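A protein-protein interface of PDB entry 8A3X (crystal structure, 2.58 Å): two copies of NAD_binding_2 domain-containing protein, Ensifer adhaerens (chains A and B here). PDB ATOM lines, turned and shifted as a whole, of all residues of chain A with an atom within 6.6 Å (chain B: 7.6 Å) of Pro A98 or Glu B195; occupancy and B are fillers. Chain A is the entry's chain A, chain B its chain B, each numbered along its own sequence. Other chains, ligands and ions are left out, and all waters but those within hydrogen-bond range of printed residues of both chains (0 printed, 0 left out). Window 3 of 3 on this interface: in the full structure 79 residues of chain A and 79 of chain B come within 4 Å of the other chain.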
ATOM      1  N   GLY A  96      -6.958  -0.854  -1.063  1.00  0.00           N
ATOM      2  CA  GLY A  96      -8.222  -1.118  -0.352  1.00  0.00           C
ATOM      3  C   GLY A  96      -9.379  -0.292  -0.885  1.00  0.00           C
ATOM      4  O   GLY A  96      -9.170   0.462  -1.840  1.00  0.00           O
ATOM      5  N   THR A  97     -10.556  -0.440  -0.266  1.00  0.00           N
ATOM      6  CA  THR A  97     -11.819   0.238  -0.649  1.00  0.00           C
ATOM      7  C   THR A  97     -11.938   1.521   0.157  1.00  0.00           C
ATOM      8  O   THR A  97     -11.261   1.673   1.160  1.00  0.00           O
ATOM      9  CB  THR A  97     -13.029  -0.678  -0.426  1.00  0.00           C
ATOM     10  OG1 THR A  97     -13.233  -0.831   0.976  1.00  0.00           O
ATOM     11  CG2 THR A  97     -12.856  -2.049  -1.044  1.00  0.00           C
ATOM     12  N   PRO A  98     -12.783   2.491  -0.249  1.00  0.00           N
ATOM     13  CA  PRO A  98     -12.971   3.712   0.536  1.00  0.00           C
ATOM     14  C   PRO A  98     -13.624   3.447   1.908  1.00  0.00           C
ATOM     15  O   PRO A  98     -13.254   4.097   2.860  1.00  0.00           O
ATOM     16  CB  PRO A  98     -13.864   4.596  -0.359  1.00  0.00           C
ATOM     17  CG  PRO A  98     -13.751   3.977  -1.738  1.00  0.00           C
ATOM     18  CD  PRO A  98     -13.571   2.493  -1.491  1.00  0.00           C
ATOM     19  N   GLU A  99     -14.570   2.508   1.991  1.00  0.00           N
ATOM     20  CA  GLU A  99     -15.198   2.111   3.278  1.00  0.00           C
ATOM     21  C   GLU A  99     -14.090   1.550   4.184  1.00  0.00           C
ATOM     22  O   GLU A  99     -14.062   1.913   5.375  1.00  0.00           O
ATOM     23  CB  GLU A  99     -16.357   1.130   3.059  1.00  0.00           C
ATOM     24  CG  GLU A  99     -17.574   1.447   3.917  1.00  0.00           C
ATOM     25  CD  GLU A  99     -18.442   0.257   4.304  1.00  0.00           C
ATOM     26  OE1 GLU A  99     -18.948  -0.434   3.390  1.00  0.00           O
ATOM     27  OE2 GLU A  99     -18.613   0.022   5.524  1.00  0.00           O
ATOM     28  N   GLY A 100     -13.186   0.739   3.623  1.00  0.00           N
ATOM     29  CA  GLY A 100     -12.007   0.176   4.316  1.00  0.00           C
ATOM     30  C   GLY A 100     -11.116   1.255   4.927  1.00  0.00           C
ATOM     31  O   GLY A 100     -10.592   1.031   6.032  1.00  0.00           O
ATOM     32  N   ALA A 101     -10.921   2.383   4.237  1.00  0.00           N
ATOM     33  CA  ALA A 101     -10.142   3.549   4.722  1.00  0.00           C
ATOM     34  C   ALA A 101     -10.884   4.191   5.895  1.00  0.00           C
ATOM     35  O   ALA A 101     -10.230   4.478   6.901  1.00  0.00           O
ATOM     36  CB  ALA A 101      -9.912   4.545   3.614  1.00  0.00           C
ATOM     37  N   ARG A 102     -12.200   4.385   5.771  1.00  0.00           N
ATOM     38  CA  ARG A 102     -13.054   5.058   6.788  1.00  0.00           C
ATOM     39  C   ARG A 102     -13.084   4.223   8.075  1.00  0.00           C
ATOM     40  O   ARG A 102     -13.050   4.834   9.153  1.00  0.00           O
ATOM     41  CB  ARG A 102     -14.452   5.310   6.217  1.00  0.00           C
ATOM     42  CG  ARG A 102     -14.450   6.292   5.053  1.00  0.00           C
ATOM     43  CD  ARG A 102     -15.823   6.791   4.640  1.00  0.00           C
ATOM     44  NE  ARG A 102     -16.330   6.182   3.412  1.00  0.00           N
ATOM     45  CZ  ARG A 102     -16.055   6.591   2.169  1.00  0.00           C
ATOM     46  NH1 ARG A 102     -16.595   5.965   1.139  1.00  0.00           N
ATOM     47  NH2 ARG A 102     -15.235   7.602   1.941  1.00  0.00           N
ATOM     48  N   GLU A 103     -13.113   2.892   7.951  1.00  0.00           N
ATOM     49  CA  GLU A 103     -13.109   1.948   9.103  1.00  0.00           C
ATOM     50  C   GLU A 103     -11.741   2.010   9.794  1.00  0.00           C
ATOM     51  O   GLU A 103     -11.710   2.246  11.005  1.00  0.00           O
ATOM     52  CB  GLU A 103     -13.446   0.518   8.664  1.00  0.00           C
ATOM     53  CG  GLU A 103     -14.331  -0.229   9.668  1.00  0.00           C
ATOM     54  CD  GLU A 103     -13.711  -0.649  10.994  1.00  0.00           C
ATOM     55  OE1 GLU A 103     -12.916  -1.605  10.995  1.00  0.00           O
ATOM     56  OE2 GLU A 103     -14.051  -0.042  12.033  1.00  0.00           O
ATOM     57  N   GLU A 163     -11.244  13.801   3.993  1.00  0.00           N
ATOM     58  CA  GLU A 163     -12.036  12.543   3.897  1.00  0.00           C
ATOM     59  C   GLU A 163     -11.088  11.407   3.498  1.00  0.00           C
ATOM     60  O   GLU A 163     -10.495  11.452   2.421  1.00  0.00           O
ATOM     61  CB  GLU A 163     -13.197  12.753   2.921  1.00  0.00           C
ATOM     62  CG  GLU A 163     -14.390  11.869   3.226  1.00  0.00           C
ATOM     63  CD  GLU A 163     -14.069  10.390   3.099  1.00  0.00           C
ATOM     64  OE1 GLU A 163     -13.635   9.975   1.992  1.00  0.00           O
ATOM     65  OE2 GLU A 163     -14.225   9.657   4.100  1.00  0.00           O
ATOM     66  N   PRO A 164     -10.863  10.393   4.369  1.00  0.00           N
ATOM     67  CA  PRO A 164      -9.805   9.402   4.150  1.00  0.00           C
ATOM     68  C   PRO A 164     -10.048   8.313   3.089  1.00  0.00           C
ATOM     69  O   PRO A 164      -9.107   7.661   2.685  1.00  0.00           O
ATOM     70  CB  PRO A 164      -9.666   8.756   5.532  1.00  0.00           C
ATOM     71  CG  PRO A 164     -11.042   8.859   6.127  1.00  0.00           C
ATOM     72  CD  PRO A 164     -11.558  10.197   5.648  1.00  0.00           C
ATOM     73  N   GLY A 165     -11.289   8.148   2.643  1.00  0.00           N
ATOM     74  CA  GLY A 165     -11.642   7.235   1.533  1.00  0.00           C
ATOM     75  C   GLY A 165     -11.212   7.758   0.161  1.00  0.00           C
ATOM     76  O   GLY A 165     -11.112   6.930  -0.765  1.00  0.00           O
ATOM     77  N   LEU A 166     -10.979   9.070   0.030  1.00  0.00           N
ATOM     78  CA  LEU A 166     -10.754   9.767  -1.270  1.00  0.00           C
ATOM     79  C   LEU A 166      -9.623   9.079  -2.056  1.00  0.00           C
ATOM     80  O   LEU A 166      -9.812   8.825  -3.258  1.00  0.00           O
ATOM     81  CB  LEU A 166     -10.448  11.247  -1.023  1.00  0.00           C
ATOM     82  CG  LEU A 166     -11.286  12.231  -1.848  1.00  0.00           C
ATOM     83  CD1 LEU A 166     -12.520  12.687  -1.073  1.00  0.00           C
ATOM     84  CD2 LEU A 166     -10.463  13.444  -2.278  1.00  0.00           C
ATOM     85  N   ASN A 168      -8.446   5.951  -2.057  1.00  0.00           N
ATOM     86  CA  ASN A 168      -8.824   4.624  -2.610  1.00  0.00           C
ATOM     87  C   ASN A 168      -9.871   4.757  -3.727  1.00  0.00           C
ATOM     88  O   ASN A 168      -9.803   3.970  -4.684  1.00  0.00           O
ATOM     89  CB  ASN A 168      -9.291   3.694  -1.497  1.00  0.00           C
ATOM     90  CG  ASN A 168      -8.137   3.252  -0.630  1.00  0.00           C
ATOM     91  OD1 ASN A 168      -6.996   3.217  -1.082  1.00  0.00           O
ATOM     92  ND2 ASN A 168      -8.434   2.899   0.608  1.00  0.00           N
ATOM     93  N   ALA A 169     -10.820   5.684  -3.619  1.00  0.00           N
ATOM     94  CA  ALA A 169     -11.814   5.949  -4.683  1.00  0.00           C
ATOM     95  C   ALA A 169     -11.052   6.230  -5.981  1.00  0.00           C
ATOM     96  O   ALA A 169     -11.245   5.483  -6.960  1.00  0.00           O
ATOM     97  CB  ALA A 169     -12.715   7.097  -4.299  1.00  0.00           C
ATOM     98  N   LEU A 170     -10.179   7.238  -5.939  1.00  0.00           N
ATOM     99  CA  LEU A 170      -9.281   7.677  -7.046  1.00  0.00           C
ATOM    100  C   LEU A 170      -8.429   6.498  -7.532  1.00  0.00           C
ATOM    101  O   LEU A 170      -8.281   6.336  -8.765  1.00  0.00           O
ATOM    102  CB  LEU A 170      -8.376   8.807  -6.540  1.00  0.00           C
ATOM    103  CG  LEU A 170      -8.163   9.999  -7.472  1.00  0.00           C
ATOM    104  CD1 LEU A 170      -8.587   9.684  -8.906  1.00  0.00           C
ATOM    105  CD2 LEU A 170      -8.900  11.239  -6.944  1.00  0.00           C
ATOM    106  N   SER A 172      -9.069   3.305  -7.494  1.00  0.00           N
ATOM    107  CA  SER A 172      -9.935   2.357  -8.243  1.00  0.00           C
ATOM    108  C   SER A 172     -10.181   2.874  -9.665  1.00  0.00           C
ATOM    109  O   SER A 172     -10.106   2.046 -10.598  1.00  0.00           O
ATOM    110  CB  SER A 172     -11.234   2.092  -7.515  1.00  0.00           C
ATOM    111  OG  SER A 172     -11.147   0.907  -6.744  1.00  0.00           O
ATOM    112  N   ILE B 189     -14.182   6.385 -15.743  1.00  0.00           N
ATOM    113  CA  ILE B 189     -15.208   7.471 -15.689  1.00  0.00           C
ATOM    114  C   ILE B 189     -16.412   6.996 -14.868  1.00  0.00           C
ATOM    115  O   ILE B 189     -16.960   7.809 -14.103  1.00  0.00           O
ATOM    116  CB  ILE B 189     -15.607   7.929 -17.108  1.00  0.00           C
ATOM    117  CG1 ILE B 189     -14.448   8.660 -17.790  1.00  0.00           C
ATOM    118  CG2 ILE B 189     -16.880   8.765 -17.097  1.00  0.00           C
ATOM    119  CD1 ILE B 189     -14.626   8.831 -19.281  1.00  0.00           C
ATOM    120  N   ALA B 190     -16.833   5.740 -15.039  1.00  0.00           N
ATOM    121  CA  ALA B 190     -18.024   5.181 -14.349  1.00  0.00           C
ATOM    122  C   ALA B 190     -17.759   5.125 -12.842  1.00  0.00           C
ATOM    123  O   ALA B 190     -18.678   5.430 -12.070  1.00  0.00           O
ATOM    124  CB  ALA B 190     -18.372   3.830 -14.901  1.00  0.00           C
ATOM    125  N   VAL B 191     -16.532   4.757 -12.466  1.00  0.00           N
ATOM    126  CA  VAL B 191     -16.029   4.746 -11.059  1.00  0.00           C
ATOM    127  C   VAL B 191     -16.064   6.174 -10.511  1.00  0.00           C
ATOM    128  O   VAL B 191     -16.730   6.393  -9.497  1.00  0.00           O
ATOM    129  CB  VAL B 191     -14.623   4.135 -10.961  1.00  0.00           C
ATOM    130  CG1 VAL B 191     -13.991   4.387  -9.607  1.00  0.00           C
ATOM    131  CG2 VAL B 191     -14.655   2.649 -11.283  1.00  0.00           C
ATOM    132  N   CYS B 192     -15.386   7.111 -11.165  1.00  0.00           N
ATOM    133  CA  CYS B 192     -15.377   8.551 -10.797  1.00  0.00           C
ATOM    134  C   CYS B 192     -16.806   9.065 -10.592  1.00  0.00           C
ATOM    135  O   CYS B 192     -17.031   9.770  -9.597  1.00  0.00           O
ATOM    136  CB  CYS B 192     -14.650   9.393 -11.839  1.00  0.00           C
ATOM    137  SG  CYS B 192     -12.862   9.113 -11.785  1.00  0.00           S
ATOM    138  N   ARG B 193     -17.730   8.741 -11.493  1.00  0.00           N
ATOM    139  CA  ARG B 193     -19.141   9.200 -11.406  1.00  0.00           C
ATOM    140  C   ARG B 193     -19.740   8.674 -10.091  1.00  0.00           C
ATOM    141  O   ARG B 193     -20.415   9.461  -9.391  1.00  0.00           O
ATOM    142  CB  ARG B 193     -19.933   8.740 -12.636  1.00  0.00           C
ATOM    143  CG  ARG B 193     -20.199   9.826 -13.673  1.00  0.00           C
ATOM    144  CD  ARG B 193     -18.975  10.283 -14.436  1.00  0.00           C
ATOM    145  NE  ARG B 193     -19.168  11.563 -15.109  1.00  0.00           N
ATOM    146  CZ  ARG B 193     -19.701  11.733 -16.323  1.00  0.00           C
ATOM    147  NH1 ARG B 193     -20.140  10.702 -17.037  1.00  0.00           N
ATOM    148  NH2 ARG B 193     -19.774  12.954 -16.823  1.00  0.00           N
ATOM    149  N   ALA B 194     -19.456   7.413  -9.758  1.00  0.00           N
ATOM    150  CA  ALA B 194     -20.023   6.697  -8.590  1.00  0.00           C
ATOM    151  C   ALA B 194     -19.451   7.234  -7.272  1.00  0.00           C
ATOM    152  O   ALA B 194     -20.226   7.303  -6.303  1.00  0.00           O
ATOM    153  CB  ALA B 194     -19.758   5.219  -8.722  1.00  0.00           C
ATOM    154  N   GLU B 195     -18.154   7.575  -7.234  1.00  0.00           N
ATOM    155  CA  GLU B 195     -17.419   8.053  -6.024  1.00  0.00           C
ATOM    156  C   GLU B 195     -17.329   9.590  -6.031  1.00  0.00           C
ATOM    157  O   GLU B 195     -16.373  10.126  -5.424  1.00  0.00           O
ATOM    158  CB  GLU B 195     -16.020   7.433  -5.967  1.00  0.00           C
ATOM    159  CG  GLU B 195     -16.018   5.921  -6.054  1.00  0.00           C
ATOM    160  CD  GLU B 195     -16.700   5.227  -4.886  1.00  0.00           C
ATOM    161  OE1 GLU B 195     -17.753   4.578  -5.088  1.00  0.00           O
ATOM    162  OE2 GLU B 195     -16.180   5.346  -3.768  1.00  0.00           O
ATOM    163  N   GLU B 196     -18.270  10.263  -6.707  1.00  0.00           N
ATOM    164  CA  GLU B 196     -18.374  11.748  -6.812  1.00  0.00           C
ATOM    165  C   GLU B 196     -16.980  12.379  -7.013  1.00  0.00           C
ATOM    166  O   GLU B 196     -16.650  13.348  -6.310  1.00  0.00           O
ATOM    167  CB  GLU B 196     -19.075  12.330  -5.569  1.00  0.00           C
ATOM    168  CG  GLU B 196     -20.581  12.555  -5.683  1.00  0.00           C
ATOM    169  CD  GLU B 196     -21.114  13.314  -6.895  1.00  0.00           C
ATOM    170  OE1 GLU B 196     -21.973  14.238  -6.723  1.00  0.00           O
ATOM    171  OE2 GLU B 196     -20.695  12.965  -8.017  1.00  0.00           O
ATOM    172  N   ILE B 197     -16.177  11.853  -7.938  1.00  0.00           N
ATOM    173  CA  ILE B 197     -14.871  12.452  -8.365  1.00  0.00           C
ATOM    174  C   ILE B 197     -15.080  13.272  -9.650  1.00  0.00           C
ATOM    175  O   ILE B 197     -15.551  12.699 -10.649  1.00  0.00           O
ATOM    176  CB  ILE B 197     -13.798  11.370  -8.588  1.00  0.00           C
ATOM    177  CG1 ILE B 197     -13.597  10.459  -7.379  1.00  0.00           C
ATOM    178  CG2 ILE B 197     -12.503  12.004  -9.023  1.00  0.00           C
ATOM    179  CD1 ILE B 197     -12.734   9.249  -7.670  1.00  0.00           C
ATOM    180  N   ASP B 198     -14.716  14.559  -9.637  1.00  0.00           N
ATOM    181  CA  ASP B 198     -14.677  15.439 -10.845  1.00  0.00           C
ATOM    182  C   ASP B 198     -13.716  14.809 -11.871  1.00  0.00           C
ATOM    183  O   ASP B 198     -12.605  14.419 -11.486  1.00  0.00           O
ATOM    184  CB  ASP B 198     -14.281  16.874 -10.477  1.00  0.00           C
ATOM    185  CG  ASP B 198     -14.022  17.772 -11.683  1.00  0.00           C
ATOM    186  OD1 ASP B 198     -15.015  18.201 -12.319  1.00  0.00           O
ATOM    187  OD2 ASP B 198     -12.822  18.023 -11.996  1.00  0.00           O
ATOM    188  N   HIS B 248     -11.579  -5.072  -5.557  1.00  0.00           N
ATOM    189  CA  HIS B 248     -12.148  -3.801  -5.033  1.00  0.00           C
ATOM    190  C   HIS B 248     -12.922  -3.111  -6.170  1.00  0.00           C
ATOM    191  O   HIS B 248     -13.942  -2.460  -5.888  1.00  0.00           O
ATOM    192  CB  HIS B 248     -11.038  -2.981  -4.345  1.00  0.00           C
ATOM    193  CG  HIS B 248     -10.238  -3.763  -3.334  1.00  0.00           C
ATOM    194  ND1 HIS B 248      -8.847  -3.712  -3.265  1.00  0.00           N
ATOM    195  CD2 HIS B 248     -10.613  -4.647  -2.379  1.00  0.00           C
ATOM    196  CE1 HIS B 248      -8.410  -4.511  -2.314  1.00  0.00           C
ATOM    197  NE2 HIS B 248      -9.474  -5.093  -1.752  1.00  0.00           N
ATOM    198  N   LEU B 252     -17.118  -2.779  -6.445  1.00  0.00           N
ATOM    199  CA  LEU B 252     -17.607  -1.388  -6.682  1.00  0.00           C
ATOM    200  C   LEU B 252     -18.608  -1.382  -7.845  1.00  0.00           C
ATOM    201  O   LEU B 252     -19.665  -0.729  -7.722  1.00  0.00           O
ATOM    202  CB  LEU B 252     -16.408  -0.477  -6.973  1.00  0.00           C
ATOM    203  CG  LEU B 252     -16.743   0.967  -7.341  1.00  0.00           C
ATOM    204  CD1 LEU B 252     -17.541   1.616  -6.226  1.00  0.00           C
ATOM    205  CD2 LEU B 252     -15.483   1.750  -7.644  1.00  0.00           C
ATOM    206  N   ALA B 255     -21.879  -3.232  -7.001  1.00  0.00           N
ATOM    207  CA  ALA B 255     -22.632  -2.363  -6.067  1.00  0.00           C
ATOM    208  C   ALA B 255     -23.291  -1.210  -6.827  1.00  0.00           C
ATOM    209  O   ALA B 255     -24.410  -0.831  -6.449  1.00  0.00           O
ATOM    210  CB  ALA B 255     -21.710  -1.848  -4.991  1.00  0.00           C
ATOM    211  N   ARG B 256     -22.617  -0.667  -7.849  1.00  0.00           N
ATOM    212  CA  ARG B 256     -23.044   0.576  -8.548  1.00  0.00           C
ATOM    213  C   ARG B 256     -23.775   0.243  -9.856  1.00  0.00           C
ATOM    214  O   ARG B 256     -24.055   1.192 -10.612  1.00  0.00           O
ATOM    215  CB  ARG B 256     -21.833   1.480  -8.789  1.00  0.00           C
ATOM    216  CG  ARG B 256     -21.219   2.079  -7.532  1.00  0.00           C
ATOM    217  CD  ARG B 256     -22.195   2.902  -6.704  1.00  0.00           C
ATOM    218  NE  ARG B 256     -21.577   3.470  -5.510  1.00  0.00           N
ATOM    219  CZ  ARG B 256     -21.933   4.619  -4.934  1.00  0.00           C
ATOM    220  NH1 ARG B 256     -22.932   5.338  -5.428  1.00  0.00           N
ATOM    221  NH2 ARG B 256     -21.286   5.028  -3.851  1.00  0.00           N
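The side-chain carboxylate (OE1) of Glu B195 lies within salt-bridge range of the guanidinium group (NH2) of Arg B256 (3.8 Å). The backbone carbonyl oxygen (O) of Thr A97 lies within hydrogen-bond range of the side-chain amide nitrogen (ND2) of Asn A168. The backbone carbonyl oxygen (O) of Cys B192 sits at hydrogen-bond distance from the backbone NH (N) of Ile B197. N of Gly A100 lies within hydrogen-bond range of OG1 of Thr A97 (3.1 Å).
Among the printed residues, pairs that only touch across the chains: Gly A96 with His B248 (3.9 Å), Thr A97 with His B248 (3.7 Å), Pro A98 with Glu B195 (3.4 Å), Ala A169 with Val B191 (3.97 Å), Ala A169 with Glu B195 (3.7 Å), Ala A169 with Ile B197 (3.8 Å) and Leu A170 with Ile B197 (3.7 Å).
Pro A98 touches just one residue of chain B: Glu B195. Of chain A, only Pro A98 (3.4 Å) and Ala A169 (3.7 Å) come within 4 Å of Glu B195. Printed residues of chain B within 4 Å of Gly A96: His B248 (3.9 Å). Printed residues of chain B within 4 Å of Ala A169: Val B191, Glu B195 and Ile B197. Of the printed residues of chain A, Val B191 touches Ala A169. Of the printed residues of chain A, Ile B197 touches Ala A169 (3.8 Å) and Leu A170 (3.7 Å). Of the printed residues of chain A, His B248 touches Gly A96 (3.9 Å) and Thr A97 (3.7 Å). Arg B193 touches none of the printed residues of chain A. Glu A103 touches none of the printed residues of chain B. The nearest residue of chain B that does not touch Pro A98 is Leu B252 (6.2 Å). The nearest residue of chain A that does not touch Glu B195 is Arg A102 (5.0 Å). The nearest printed residue of chain A that does not touch Ile B197 is Leu A166 (5.3 Å).
Hydrophobic or aromatic side chains of chain B that line the printed part of chain A: Val B191, Ile B197 and His B248. Among the printed residues, no Asp or Glu carboxylate lies within 4 Å of a Lys or Arg side-chain nitrogen of the other chain.
No position is printed for both chains.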
